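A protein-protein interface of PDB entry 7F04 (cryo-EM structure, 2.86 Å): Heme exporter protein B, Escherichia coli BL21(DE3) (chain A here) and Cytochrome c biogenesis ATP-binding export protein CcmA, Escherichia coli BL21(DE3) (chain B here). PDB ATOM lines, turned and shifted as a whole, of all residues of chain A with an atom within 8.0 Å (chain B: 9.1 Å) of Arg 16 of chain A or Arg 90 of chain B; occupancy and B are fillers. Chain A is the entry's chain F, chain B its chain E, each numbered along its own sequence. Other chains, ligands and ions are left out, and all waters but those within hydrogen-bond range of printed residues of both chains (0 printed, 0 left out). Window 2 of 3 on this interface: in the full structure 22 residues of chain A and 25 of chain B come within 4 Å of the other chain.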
ATOM      1  N   LEU A   9      -5.820  -3.575  16.521  1.00  0.00           N
ATOM      2  CA  LEU A   9      -5.773  -2.334  17.284  1.00  0.00           C
ATOM      3  C   LEU A   9      -5.396  -2.595  18.734  1.00  0.00           C
ATOM      4  O   LEU A   9      -4.587  -1.862  19.313  1.00  0.00           O
ATOM      5  CB  LEU A   9      -7.115  -1.612  17.208  1.00  0.00           C
ATOM      6  CG  LEU A   9      -7.136  -0.234  17.869  1.00  0.00           C
ATOM      7  CD1 LEU A   9      -6.757   0.846  16.871  1.00  0.00           C
ATOM      8  CD2 LEU A   9      -8.492   0.050  18.490  1.00  0.00           C
ATOM      9  N   GLU A  10      -5.978  -3.628  19.344  1.00  0.00           N
ATOM     10  CA  GLU A  10      -5.632  -3.940  20.726  1.00  0.00           C
ATOM     11  C   GLU A  10      -4.191  -4.417  20.837  1.00  0.00           C
ATOM     12  O   GLU A  10      -3.499  -4.089  21.808  1.00  0.00           O
ATOM     13  CB  GLU A  10      -6.596  -4.979  21.292  1.00  0.00           C
ATOM     14  CG  GLU A  10      -8.043  -4.531  21.315  1.00  0.00           C
ATOM     15  CD  GLU A  10      -8.227  -3.190  21.995  1.00  0.00           C
ATOM     16  OE1 GLU A  10      -7.700  -3.011  23.113  1.00  0.00           O
ATOM     17  OE2 GLU A  10      -8.899  -2.314  21.411  1.00  0.00           O
ATOM     18  N   LEU A  11      -3.716  -5.185  19.852  1.00  0.00           N
ATOM     19  CA  LEU A  11      -2.312  -5.589  19.847  1.00  0.00           C
ATOM     20  C   LEU A  11      -1.393  -4.376  19.789  1.00  0.00           C
ATOM     21  O   LEU A  11      -0.406  -4.291  20.530  1.00  0.00           O
ATOM     22  CB  LEU A  11      -2.036  -6.516  18.664  1.00  0.00           C
ATOM     23  CG  LEU A  11      -2.167  -8.018  18.887  1.00  0.00           C
ATOM     24  CD1 LEU A  11      -1.697  -8.755  17.652  1.00  0.00           C
ATOM     25  CD2 LEU A  11      -1.368  -8.443  20.100  1.00  0.00           C
ATOM     26  N   ARG A  12      -1.705  -3.426  18.907  1.00  0.00           N
ATOM     27  CA  ARG A  12      -0.883  -2.230  18.769  1.00  0.00           C
ATOM     28  C   ARG A  12      -0.919  -1.377  20.028  1.00  0.00           C
ATOM     29  O   ARG A  12       0.103  -0.813  20.432  1.00  0.00           O
ATOM     30  CB  ARG A  12      -1.344  -1.425  17.557  1.00  0.00           C
ATOM     31  CG  ARG A  12      -0.519  -0.193  17.279  1.00  0.00           C
ATOM     32  CD  ARG A  12      -0.994   0.497  16.023  1.00  0.00           C
ATOM     33  NE  ARG A  12      -0.722  -0.306  14.839  1.00  0.00           N
ATOM     34  CZ  ARG A  12      -1.176  -0.028  13.625  1.00  0.00           C
ATOM     35  NH1 ARG A  12      -1.946   1.022  13.399  1.00  0.00           N
ATOM     36  NH2 ARG A  12      -0.846  -0.825  12.612  1.00  0.00           N
ATOM     37  N   VAL A  13      -2.089  -1.261  20.658  1.00  0.00           N
ATOM     38  CA  VAL A  13      -2.193  -0.498  21.899  1.00  0.00           C
ATOM     39  C   VAL A  13      -1.368  -1.156  22.997  1.00  0.00           C
ATOM     40  O   VAL A  13      -0.664  -0.478  23.754  1.00  0.00           O
ATOM     41  CB  VAL A  13      -3.669  -0.347  22.309  1.00  0.00           C
ATOM     42  CG1 VAL A  13      -3.780   0.068  23.762  1.00  0.00           C
ATOM     43  CG2 VAL A  13      -4.364   0.659  21.414  1.00  0.00           C
ATOM     44  N   ALA A  14      -1.440  -2.485  23.101  1.00  0.00           N
ATOM     45  CA  ALA A  14      -0.680  -3.192  24.126  1.00  0.00           C
ATOM     46  C   ALA A  14       0.819  -3.064  23.897  1.00  0.00           C
ATOM     47  O   ALA A  14       1.588  -2.931  24.855  1.00  0.00           O
ATOM     48  CB  ALA A  14      -1.090  -4.662  24.163  1.00  0.00           C
ATOM     49  N   PHE A  15       1.257  -3.112  22.637  1.00  0.00           N
ATOM     50  CA  PHE A  15       2.686  -3.019  22.354  1.00  0.00           C
ATOM     51  C   PHE A  15       3.259  -1.674  22.773  1.00  0.00           C
ATOM     52  O   PHE A  15       4.391  -1.608  23.262  1.00  0.00           O
ATOM     53  CB  PHE A  15       2.944  -3.267  20.869  1.00  0.00           C
ATOM     54  CG  PHE A  15       3.051  -4.717  20.510  1.00  0.00           C
ATOM     55  CD1 PHE A  15       3.618  -5.621  21.388  1.00  0.00           C
ATOM     56  CD2 PHE A  15       2.580  -5.179  19.293  1.00  0.00           C
ATOM     57  CE1 PHE A  15       3.717  -6.955  21.062  1.00  0.00           C
ATOM     58  CE2 PHE A  15       2.676  -6.513  18.961  1.00  0.00           C
ATOM     59  CZ  PHE A  15       3.245  -7.403  19.847  1.00  0.00           C
ATOM     60  N   ARG A  16       2.505  -0.595  22.586  1.00  0.00           N
ATOM     61  CA  ARG A  16       2.955   0.730  22.987  1.00  0.00           C
ATOM     62  C   ARG A  16       2.752   1.002  24.468  1.00  0.00           C
ATOM     63  O   ARG A  16       3.285   1.992  24.978  1.00  0.00           O
ATOM     64  CB  ARG A  16       2.246   1.797  22.150  1.00  0.00           C
ATOM     65  CG  ARG A  16       2.668   1.748  20.697  1.00  0.00           C
ATOM     66  CD  ARG A  16       1.984   2.786  19.848  1.00  0.00           C
ATOM     67  NE  ARG A  16       2.416   2.671  18.462  1.00  0.00           N
ATOM     68  CZ  ARG A  16       1.951   3.410  17.466  1.00  0.00           C
ATOM     69  NH1 ARG A  16       1.035   4.342  17.668  1.00  0.00           N
ATOM     70  NH2 ARG A  16       2.416   3.209  16.238  1.00  0.00           N
ATOM     71  N   HIS A  17       1.999   0.159  25.166  1.00  0.00           N
ATOM     72  CA  HIS A  17       1.954   0.182  26.626  1.00  0.00           C
ATOM     73  C   HIS A  17       2.992  -0.764  27.212  1.00  0.00           C
ATOM     74  O   HIS A  17       2.697  -1.595  28.067  1.00  0.00           O
ATOM     75  CB  HIS A  17       0.557  -0.174  27.117  1.00  0.00           C
ATOM     76  CG  HIS A  17      -0.403   0.972  27.098  1.00  0.00           C
ATOM     77  ND1 HIS A  17      -1.006   1.418  25.943  1.00  0.00           N
ATOM     78  CD2 HIS A  17      -0.863   1.765  28.094  1.00  0.00           C
ATOM     79  CE1 HIS A  17      -1.799   2.435  26.228  1.00  0.00           C
ATOM     80  NE2 HIS A  17      -1.729   2.667  27.526  1.00  0.00           N
ATOM     81  N   SER A  18       4.227  -0.643  26.738  1.00  0.00           N
ATOM     82  CA  SER A  18       5.300  -1.489  27.228  1.00  0.00           C
ATOM     83  C   SER A  18       5.662  -1.103  28.657  1.00  0.00           C
ATOM     84  O   SER A  18       5.302  -0.029  29.150  1.00  0.00           O
ATOM     85  CB  SER A  18       6.522  -1.383  26.321  1.00  0.00           C
ATOM     86  OG  SER A  18       7.565  -2.207  26.796  1.00  0.00           O
ATOM     87  N   ALA A  19       6.372  -2.009  29.330  1.00  0.00           N
ATOM     88  CA  ALA A  19       6.693  -1.970  30.754  1.00  0.00           C
ATOM     89  C   ALA A  19       5.456  -2.179  31.615  1.00  0.00           C
ATOM     90  O   ALA A  19       5.573  -2.246  32.843  1.00  0.00           O
ATOM     91  CB  ALA A  19       7.395  -0.671  31.179  1.00  0.00           C
ATOM     92  N   GLU A  20       4.275  -2.282  31.012  1.00  0.00           N
ATOM     93  CA  GLU A  20       3.065  -2.723  31.687  1.00  0.00           C
ATOM     94  C   GLU A  20       2.711  -4.158  31.337  1.00  0.00           C
ATOM     95  O   GLU A  20       2.058  -4.842  32.132  1.00  0.00           O
ATOM     96  CB  GLU A  20       1.897  -1.798  31.329  1.00  0.00           C
ATOM     97  CG  GLU A  20       0.594  -2.105  32.045  1.00  0.00           C
ATOM     98  CD  GLU A  20      -0.510  -1.128  31.692  1.00  0.00           C
ATOM     99  OE1 GLU A  20      -0.265  -0.220  30.871  1.00  0.00           O
ATOM    100  OE2 GLU A  20      -1.623  -1.269  32.236  1.00  0.00           O
ATOM    101  N   ILE A  21       3.139  -4.625  30.164  1.00  0.00           N
ATOM    102  CA  ILE A  21       3.011  -6.033  29.814  1.00  0.00           C
ATOM    103  C   ILE A  21       4.243  -6.833  30.220  1.00  0.00           C
ATOM    104  O   ILE A  21       4.171  -8.069  30.290  1.00  0.00           O
ATOM    105  CB  ILE A  21       2.743  -6.199  28.307  1.00  0.00           C
ATOM    106  CG1 ILE A  21       4.029  -6.014  27.505  1.00  0.00           C
ATOM    107  CG2 ILE A  21       1.694  -5.205  27.840  1.00  0.00           C
ATOM    108  CD1 ILE A  21       3.819  -6.057  26.012  1.00  0.00           C
ATOM    109  N   ARG A  68      -5.382  -4.228  32.588  1.00  0.00           N
ATOM    110  CA  ARG A  68      -5.401  -3.370  31.412  1.00  0.00           C
ATOM    111  C   ARG A  68      -6.316  -3.875  30.302  1.00  0.00           C
ATOM    112  O   ARG A  68      -6.267  -3.337  29.193  1.00  0.00           O
ATOM    113  CB  ARG A  68      -3.982  -3.207  30.867  1.00  0.00           C
ATOM    114  CG  ARG A  68      -3.346  -4.506  30.400  1.00  0.00           C
ATOM    115  CD  ARG A  68      -2.326  -4.266  29.300  1.00  0.00           C
ATOM    116  NE  ARG A  68      -2.887  -3.513  28.185  1.00  0.00           N
ATOM    117  CZ  ARG A  68      -3.471  -4.062  27.129  1.00  0.00           C
ATOM    118  NH1 ARG A  68      -3.585  -5.375  27.005  1.00  0.00           N
ATOM    119  NH2 ARG A  68      -3.956  -3.274  26.172  1.00  0.00           N
ATOM    120  N   ARG A  71      -9.375  -1.390  31.012  1.00  0.00           N
ATOM    121  CA  ARG A  71      -9.144  -0.253  31.895  1.00  0.00           C
ATOM    122  C   ARG A  71      -9.027   1.050  31.115  1.00  0.00           C
ATOM    123  O   ARG A  71      -9.746   2.015  31.394  1.00  0.00           O
ATOM    124  CB  ARG A  71      -7.891  -0.531  32.724  1.00  0.00           C
ATOM    125  CG  ARG A  71      -7.508   0.450  33.815  1.00  0.00           C
ATOM    126  CD  ARG A  71      -6.659   1.574  33.267  1.00  0.00           C
ATOM    127  NE  ARG A  71      -5.483   1.033  32.595  1.00  0.00           N
ATOM    128  CZ  ARG A  71      -4.374   0.643  33.206  1.00  0.00           C
ATOM    129  NH1 ARG A  71      -4.276   0.644  34.524  1.00  0.00           N
ATOM    130  NH2 ARG A  71      -3.348   0.217  32.477  1.00  0.00           N
ATOM    131  N   ASP A  72      -8.145   1.095  30.120  1.00  0.00           N
ATOM    132  CA  ASP A  72      -7.960   2.316  29.337  1.00  0.00           C
ATOM    133  C   ASP A  72      -8.906   2.357  28.144  1.00  0.00           C
ATOM    134  O   ASP A  72      -8.521   2.651  27.015  1.00  0.00           O
ATOM    135  CB  ASP A  72      -6.510   2.436  28.888  1.00  0.00           C
ATOM    136  CG  ASP A  72      -5.598   2.935  29.990  1.00  0.00           C
ATOM    137  OD1 ASP A  72      -5.940   3.950  30.632  1.00  0.00           O
ATOM    138  OD2 ASP A  72      -4.538   2.313  30.213  1.00  0.00           O
ATOM    139  N   ASP A  76     -11.814   6.783  27.785  1.00  0.00           N
ATOM    140  CA  ASP A  76     -11.907   7.362  26.450  1.00  0.00           C
ATOM    141  C   ASP A  76     -12.898   6.641  25.544  1.00  0.00           C
ATOM    142  O   ASP A  76     -13.855   7.265  25.077  1.00  0.00           O
ATOM    143  CB  ASP A  76     -10.504   7.411  25.825  1.00  0.00           C
ATOM    144  CG  ASP A  76      -9.886   6.034  25.638  1.00  0.00           C
ATOM    145  OD1 ASP A  76     -10.516   5.031  26.025  1.00  0.00           O
ATOM    146  OD2 ASP A  76      -8.757   5.953  25.114  1.00  0.00           O
ATOM    147  N   ILE B  87     -10.660   8.092  21.547  1.00  0.00           N
ATOM    148  CA  ILE B  87      -9.438   7.809  20.811  1.00  0.00           C
ATOM    149  C   ILE B  87      -8.363   7.366  21.793  1.00  0.00           C
ATOM    150  O   ILE B  87      -8.387   7.709  22.975  1.00  0.00           O
ATOM    151  CB  ILE B  87      -8.958   9.030  20.001  1.00  0.00           C
ATOM    152  CG1 ILE B  87      -8.794  10.238  20.920  1.00  0.00           C
ATOM    153  CG2 ILE B  87      -9.926   9.341  18.876  1.00  0.00           C
ATOM    154  CD1 ILE B  87      -8.217  11.439  20.236  1.00  0.00           C
ATOM    155  N   LYS B  88      -7.409   6.595  21.279  1.00  0.00           N
ATOM    156  CA  LYS B  88      -6.319   6.064  22.086  1.00  0.00           C
ATOM    157  C   LYS B  88      -5.198   7.088  22.175  1.00  0.00           C
ATOM    158  O   LYS B  88      -4.720   7.584  21.151  1.00  0.00           O
ATOM    159  CB  LYS B  88      -5.800   4.757  21.487  1.00  0.00           C
ATOM    160  CG  LYS B  88      -6.838   3.652  21.431  1.00  0.00           C
ATOM    161  CD  LYS B  88      -7.216   3.193  22.821  1.00  0.00           C
ATOM    162  CE  LYS B  88      -8.192   2.039  22.769  1.00  0.00           C
ATOM    163  NZ  LYS B  88      -8.593   1.619  24.136  1.00  0.00           N
ATOM    164  N   THR B  89      -4.778   7.399  23.403  1.00  0.00           N
ATOM    165  CA  THR B  89      -3.789   8.453  23.602  1.00  0.00           C
ATOM    166  C   THR B  89      -2.407   8.045  23.108  1.00  0.00           C
ATOM    167  O   THR B  89      -1.668   8.885  22.583  1.00  0.00           O
ATOM    168  CB  THR B  89      -3.722   8.845  25.077  1.00  0.00           C
ATOM    169  OG1 THR B  89      -3.477   7.679  25.872  1.00  0.00           O
ATOM    170  CG2 THR B  89      -5.028   9.486  25.514  1.00  0.00           C
ATOM    171  N   ARG B  90      -2.034   6.778  23.268  1.00  0.00           N
ATOM    172  CA  ARG B  90      -0.705   6.336  22.868  1.00  0.00           C
ATOM    173  C   ARG B  90      -0.571   6.116  21.368  1.00  0.00           C
ATOM    174  O   ARG B  90       0.557   5.996  20.878  1.00  0.00           O
ATOM    175  CB  ARG B  90      -0.333   5.056  23.615  1.00  0.00           C
ATOM    176  CG  ARG B  90      -0.285   5.231  25.121  1.00  0.00           C
ATOM    177  CD  ARG B  90       1.142   5.283  25.632  1.00  0.00           C
ATOM    178  NE  ARG B  90       1.212   5.013  27.063  1.00  0.00           N
ATOM    179  CZ  ARG B  90       2.311   4.639  27.702  1.00  0.00           C
ATOM    180  NH1 ARG B  90       3.460   4.481  27.067  1.00  0.00           N
ATOM    181  NH2 ARG B  90       2.255   4.418  29.012  1.00  0.00           N
ATOM    182  N   LEU B  91      -1.674   6.064  20.631  1.00  0.00           N
ATOM    183  CA  LEU B  91      -1.624   5.932  19.185  1.00  0.00           C
ATOM    184  C   LEU B  91      -1.570   7.308  18.538  1.00  0.00           C
ATOM    185  O   LEU B  91      -1.992   8.306  19.126  1.00  0.00           O
ATOM    186  CB  LEU B  91      -2.838   5.164  18.662  1.00  0.00           C
ATOM    187  CG  LEU B  91      -3.063   3.751  19.196  1.00  0.00           C
ATOM    188  CD1 LEU B  91      -4.247   3.114  18.497  1.00  0.00           C
ATOM    189  CD2 LEU B  91      -1.819   2.905  19.019  1.00  0.00           C
ATOM    190  N   THR B  92      -1.042   7.356  17.320  1.00  0.00           N
ATOM    191  CA  THR B  92      -0.970   8.616  16.604  1.00  0.00           C
ATOM    192  C   THR B  92      -2.362   9.037  16.140  1.00  0.00           C
ATOM    193  O   THR B  92      -3.331   8.278  16.216  1.00  0.00           O
ATOM    194  CB  THR B  92      -0.020   8.512  15.414  1.00  0.00           C
ATOM    195  OG1 THR B  92      -0.629   7.738  14.376  1.00  0.00           O
ATOM    196  CG2 THR B  92       1.278   7.849  15.832  1.00  0.00           C
ATOM    197  N   ALA B  93      -2.460  10.283  15.673  1.00  0.00           N
ATOM    198  CA  ALA B  93      -3.740  10.784  15.188  1.00  0.00           C
ATOM    199  C   ALA B  93      -4.203  10.015  13.959  1.00  0.00           C
ATOM    200  O   ALA B  93      -5.390   9.703  13.823  1.00  0.00           O
ATOM    201  CB  ALA B  93      -3.637  12.277  14.880  1.00  0.00           C
ATOM    202  N   LEU B  94      -3.278   9.708  13.047  1.00  0.00           N
ATOM    203  CA  LEU B  94      -3.637   8.957  11.849  1.00  0.00           C
ATOM    204  C   LEU B  94      -4.038   7.528  12.188  1.00  0.00           C
ATOM    205  O   LEU B  94      -4.976   6.987  11.597  1.00  0.00           O
ATOM    206  CB  LEU B  94      -2.475   8.969  10.858  1.00  0.00           C
ATOM    207  CG  LEU B  94      -2.619   8.097   9.612  1.00  0.00           C
ATOM    208  CD1 LEU B  94      -3.639   8.695   8.670  1.00  0.00           C
ATOM    209  CD2 LEU B  94      -1.282   7.935   8.918  1.00  0.00           C
ATOM    210  N   GLU B  95      -3.333   6.899  13.132  1.00  0.00           N
ATOM    211  CA  GLU B  95      -3.659   5.530  13.517  1.00  0.00           C
ATOM    212  C   GLU B  95      -5.028   5.449  14.175  1.00  0.00           C
ATOM    213  O   GLU B  95      -5.773   4.489  13.950  1.00  0.00           O
ATOM    214  CB  GLU B  95      -2.592   4.980  14.457  1.00  0.00           C
ATOM    215  CG  GLU B  95      -1.292   4.621  13.776  1.00  0.00           C
ATOM    216  CD  GLU B  95      -0.241   4.174  14.759  1.00  0.00           C
ATOM    217  OE1 GLU B  95      -0.571   4.046  15.954  1.00  0.00           O
ATOM    218  OE2 GLU B  95       0.914   3.957  14.342  1.00  0.00           O
ATOM    219  N   ASN B  96      -5.366   6.430  15.013  1.00  0.00           N
ATOM    220  CA  ASN B  96      -6.689   6.451  15.627  1.00  0.00           C
ATOM    221  C   ASN B  96      -7.780   6.631  14.581  1.00  0.00           C
ATOM    222  O   ASN B  96      -8.824   5.975  14.646  1.00  0.00           O
ATOM    223  CB  ASN B  96      -6.759   7.556  16.678  1.00  0.00           C
ATOM    224  CG  ASN B  96      -6.528   7.038  18.078  1.00  0.00           C
ATOM    225  OD1 ASN B  96      -7.057   5.996  18.459  1.00  0.00           O
ATOM    226  ND2 ASN B  96      -5.731   7.758  18.851  1.00  0.00           N
ATOM    227  N   GLU B 122      -0.136  14.315  12.050  1.00  0.00           N
ATOM    228  CA  GLU B 122      -0.736  13.013  11.788  1.00  0.00           C
ATOM    229  C   GLU B 122       0.086  11.875  12.381  1.00  0.00           C
ATOM    230  O   GLU B 122      -0.474  10.835  12.743  1.00  0.00           O
ATOM    231  CB  GLU B 122      -0.904  12.813  10.284  1.00  0.00           C
ATOM    232  CG  GLU B 122      -1.932  13.730   9.655  1.00  0.00           C
ATOM    233  CD  GLU B 122      -1.309  14.776   8.761  1.00  0.00           C
ATOM    234  OE1 GLU B 122      -0.090  15.014   8.884  1.00  0.00           O
ATOM    235  OE2 GLU B 122      -2.039  15.362   7.935  1.00  0.00           O
ATOM    236  N   ASP B 123       1.403  12.047  12.483  1.00  0.00           N
ATOM    237  CA  ASP B 123       2.301  11.000  12.952  1.00  0.00           C
ATOM    238  C   ASP B 123       2.786  11.253  14.375  1.00  0.00           C
ATOM    239  O   ASP B 123       3.862  10.794  14.761  1.00  0.00           O
ATOM    240  CB  ASP B 123       3.492  10.858  12.006  1.00  0.00           C
ATOM    241  CG  ASP B 123       3.129  10.156  10.714  1.00  0.00           C
ATOM    242  OD1 ASP B 123       2.339   9.190  10.762  1.00  0.00           O
ATOM    243  OD2 ASP B 123       3.634  10.570   9.650  1.00  0.00           O
ATOM    244  N   ILE B 124       2.004  11.974  15.162  1.00  0.00           N
ATOM    245  CA  ILE B 124       2.348  12.325  16.537  1.00  0.00           C
ATOM    246  C   ILE B 124       1.340  11.655  17.460  1.00  0.00           C
ATOM    247  O   ILE B 124       0.137  11.709  17.182  1.00  0.00           O
ATOM    248  CB  ILE B 124       2.353  13.851  16.751  1.00  0.00           C
ATOM    249  CG1 ILE B 124       3.437  14.502  15.894  1.00  0.00           C
ATOM    250  CG2 ILE B 124       2.556  14.191  18.214  1.00  0.00           C
ATOM    251  CD1 ILE B 124       3.606  15.981  16.135  1.00  0.00           C
ATOM    252  N   PRO B 125       1.776  11.013  18.543  1.00  0.00           N
ATOM    253  CA  PRO B 125       0.823  10.374  19.455  1.00  0.00           C
ATOM    254  C   PRO B 125      -0.161  11.376  20.034  1.00  0.00           C
ATOM    255  O   PRO B 125       0.145  12.557  20.206  1.00  0.00           O
ATOM    256  CB  PRO B 125       1.719   9.777  20.544  1.00  0.00           C
ATOM    257  CG  PRO B 125       3.024   9.570  19.873  1.00  0.00           C
ATOM    258  CD  PRO B 125       3.170  10.689  18.887  1.00  0.00           C
ATOM    259  N   VAL B 126      -1.368  10.886  20.321  1.00  0.00           N
ATOM    260  CA  VAL B 126      -2.444  11.756  20.785  1.00  0.00           C
ATOM    261  C   VAL B 126      -2.092  12.395  22.124  1.00  0.00           C
ATOM    262  O   VAL B 126      -2.363  13.580  22.346  1.00  0.00           O
ATOM    263  CB  VAL B 126      -3.767  10.972  20.853  1.00  0.00           C
ATOM    264  CG1 VAL B 126      -4.854  11.824  21.454  1.00  0.00           C
ATOM    265  CG2 VAL B 126      -4.179  10.545  19.465  1.00  0.00           C
ATOM    266  N   ASN B 127      -1.482  11.632  23.034  1.00  0.00           N
ATOM    267  CA  ASN B 127      -1.152  12.190  24.342  1.00  0.00           C
ATOM    268  C   ASN B 127      -0.131  13.316  24.249  1.00  0.00           C
ATOM    269  O   ASN B 127       0.007  14.092  25.201  1.00  0.00           O
ATOM    270  CB  ASN B 127      -0.640  11.098  25.287  1.00  0.00           C
ATOM    271  CG  ASN B 127       0.479  10.271  24.686  1.00  0.00           C
ATOM    272  OD1 ASN B 127       1.192  10.719  23.791  1.00  0.00           O
ATOM    273  ND2 ASN B 127       0.648   9.057  25.191  1.00  0.00           N
ATOM    274  N   GLN B 128       0.583  13.424  23.133  1.00  0.00           N
ATOM    275  CA  GLN B 128       1.525  14.508  22.906  1.00  0.00           C
ATOM    276  C   GLN B 128       0.894  15.699  22.202  1.00  0.00           C
ATOM    277  O   GLN B 128       1.607  16.644  21.859  1.00  0.00           O
ATOM    278  CB  GLN B 128       2.719  14.007  22.093  1.00  0.00           C
ATOM    279  CG  GLN B 128       3.439  12.833  22.722  1.00  0.00           C
ATOM    280  CD  GLN B 128       4.780  12.565  22.079  1.00  0.00           C
ATOM    281  OE1 GLN B 128       5.207  13.293  21.184  1.00  0.00           O
ATOM    282  NE2 GLN B 128       5.453  11.517  22.533  1.00  0.00           N
ATOM    283  N   GLN B 134      -6.379  17.245  20.512  1.00  0.00           N
ATOM    284  CA  GLN B 134      -6.853  15.901  20.812  1.00  0.00           C
ATOM    285  C   GLN B 134      -8.330  15.748  20.482  1.00  0.00           C
ATOM    286  O   GLN B 134      -8.770  14.659  20.102  1.00  0.00           O
ATOM    287  CB  GLN B 134      -6.606  15.572  22.281  1.00  0.00           C
ATOM    288  CG  GLN B 134      -5.185  15.167  22.595  1.00  0.00           C
ATOM    289  CD  GLN B 134      -4.986  14.844  24.056  1.00  0.00           C
ATOM    290  OE1 GLN B 134      -5.569  13.896  24.576  1.00  0.00           O
ATOM    291  NE2 GLN B 134      -4.158  15.630  24.730  1.00  0.00           N
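NZ of Lys 88 of chain B sits at hydrogen-bond distance from O of Asp 72 of chain A, 3.1 Å away. The guanidinium group (NH1) of Arg 90 of chain B lies within hydrogen-bond range of the backbone carbonyl oxygen (O) of Arg 16 of chain A (3.3 Å). OE2 of Glu 95 of chain B is in salt-bridge range of NH2 of Arg 16 of chain A (2.5 Å). O of Ile 87 of chain B sits close to OD2 of Asp 76 of chain A (2.8 Å).
The backbone carbonyl oxygen (O) of Lys 88 of chain B sits at hydrogen-bond distance from the side-chain amide nitrogen (ND2) of Asn 96 of chain B (2.5 Å). N of Val 126 of chain B sits at hydrogen-bond distance from O of Leu 91 of chain B. OG1 of Thr 92 of chain B is in hydrogen-bond range of N of Glu 95 of chain B (3.1 Å). A ring nitrogen (ND1) of His 17 of chain A is in hydrogen-bond range of the backbone carbonyl oxygen (O) of Val 13 of chain A. NE of Arg 71 of chain A is in salt-bridge range of OD2 of Asp 72 of chain A, at 2.9 Å.
CD1 of Leu 9 of chain A touches CD1 of Leu 91 of chain B (3.8 Å). Arg 12 of chain A touches Leu 91 of chain B (CG to CD2, 3.8 Å). CD of Arg 12 of chain A touches OE1 of Glu 95 of chain B, 3.6 Å away. Lys 88 of chain B touches Val 13 of chain A. CG2 of Val 13 of chain A touches CD1 of Leu 91 of chain B, at 3.8 Å. Arg 16 of chain A touches Leu 91 of chain B. Arg 16 of chain A touches Thr 92 of chain B. Arg 90 of chain B touches His 17 of chain A (CG to CE1, 3.4 Å). Lys 88 of chain B touches Asp 76 of chain A.
Of chain B, only Arg 90 (3.3 Å), Leu 91 (3.4 Å), Thr 92 (3.7 Å) and Glu 95 (2.4 Å) come within 4 Å of Arg 16 of chain A. Of chain A, only Arg 16 (3.3 Å) and His 17 (3.4 Å) come within 4 Å of Arg 90 of chain B. Of chain B, only Arg 90 (3.4 Å) comes within 4 Å of His 17 of chain A. Of the printed residues of chain A, Ile 87 of chain B touches Asp 76 (2.8 Å). Printed residues of chain A within 4 Å of Lys 88 of chain B: Val 13 (3.9 Å), Asp 72 (3.1 Å) and Asp 76 (3.9 Å). Ser 18 of chain A touches none of the printed residues of chain B. The nearest residue of chain B that does not touch Arg 16 of chain A is Pro 125 of chain B (6.0 Å). The nearest residue of chain A that does not touch Arg 90 of chain B is Ser 18 of chain A (5.2 Å). The nearest printed residue of chain B that does not touch Asp 72 of chain A is Ile 87 of chain B (6.5 Å).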
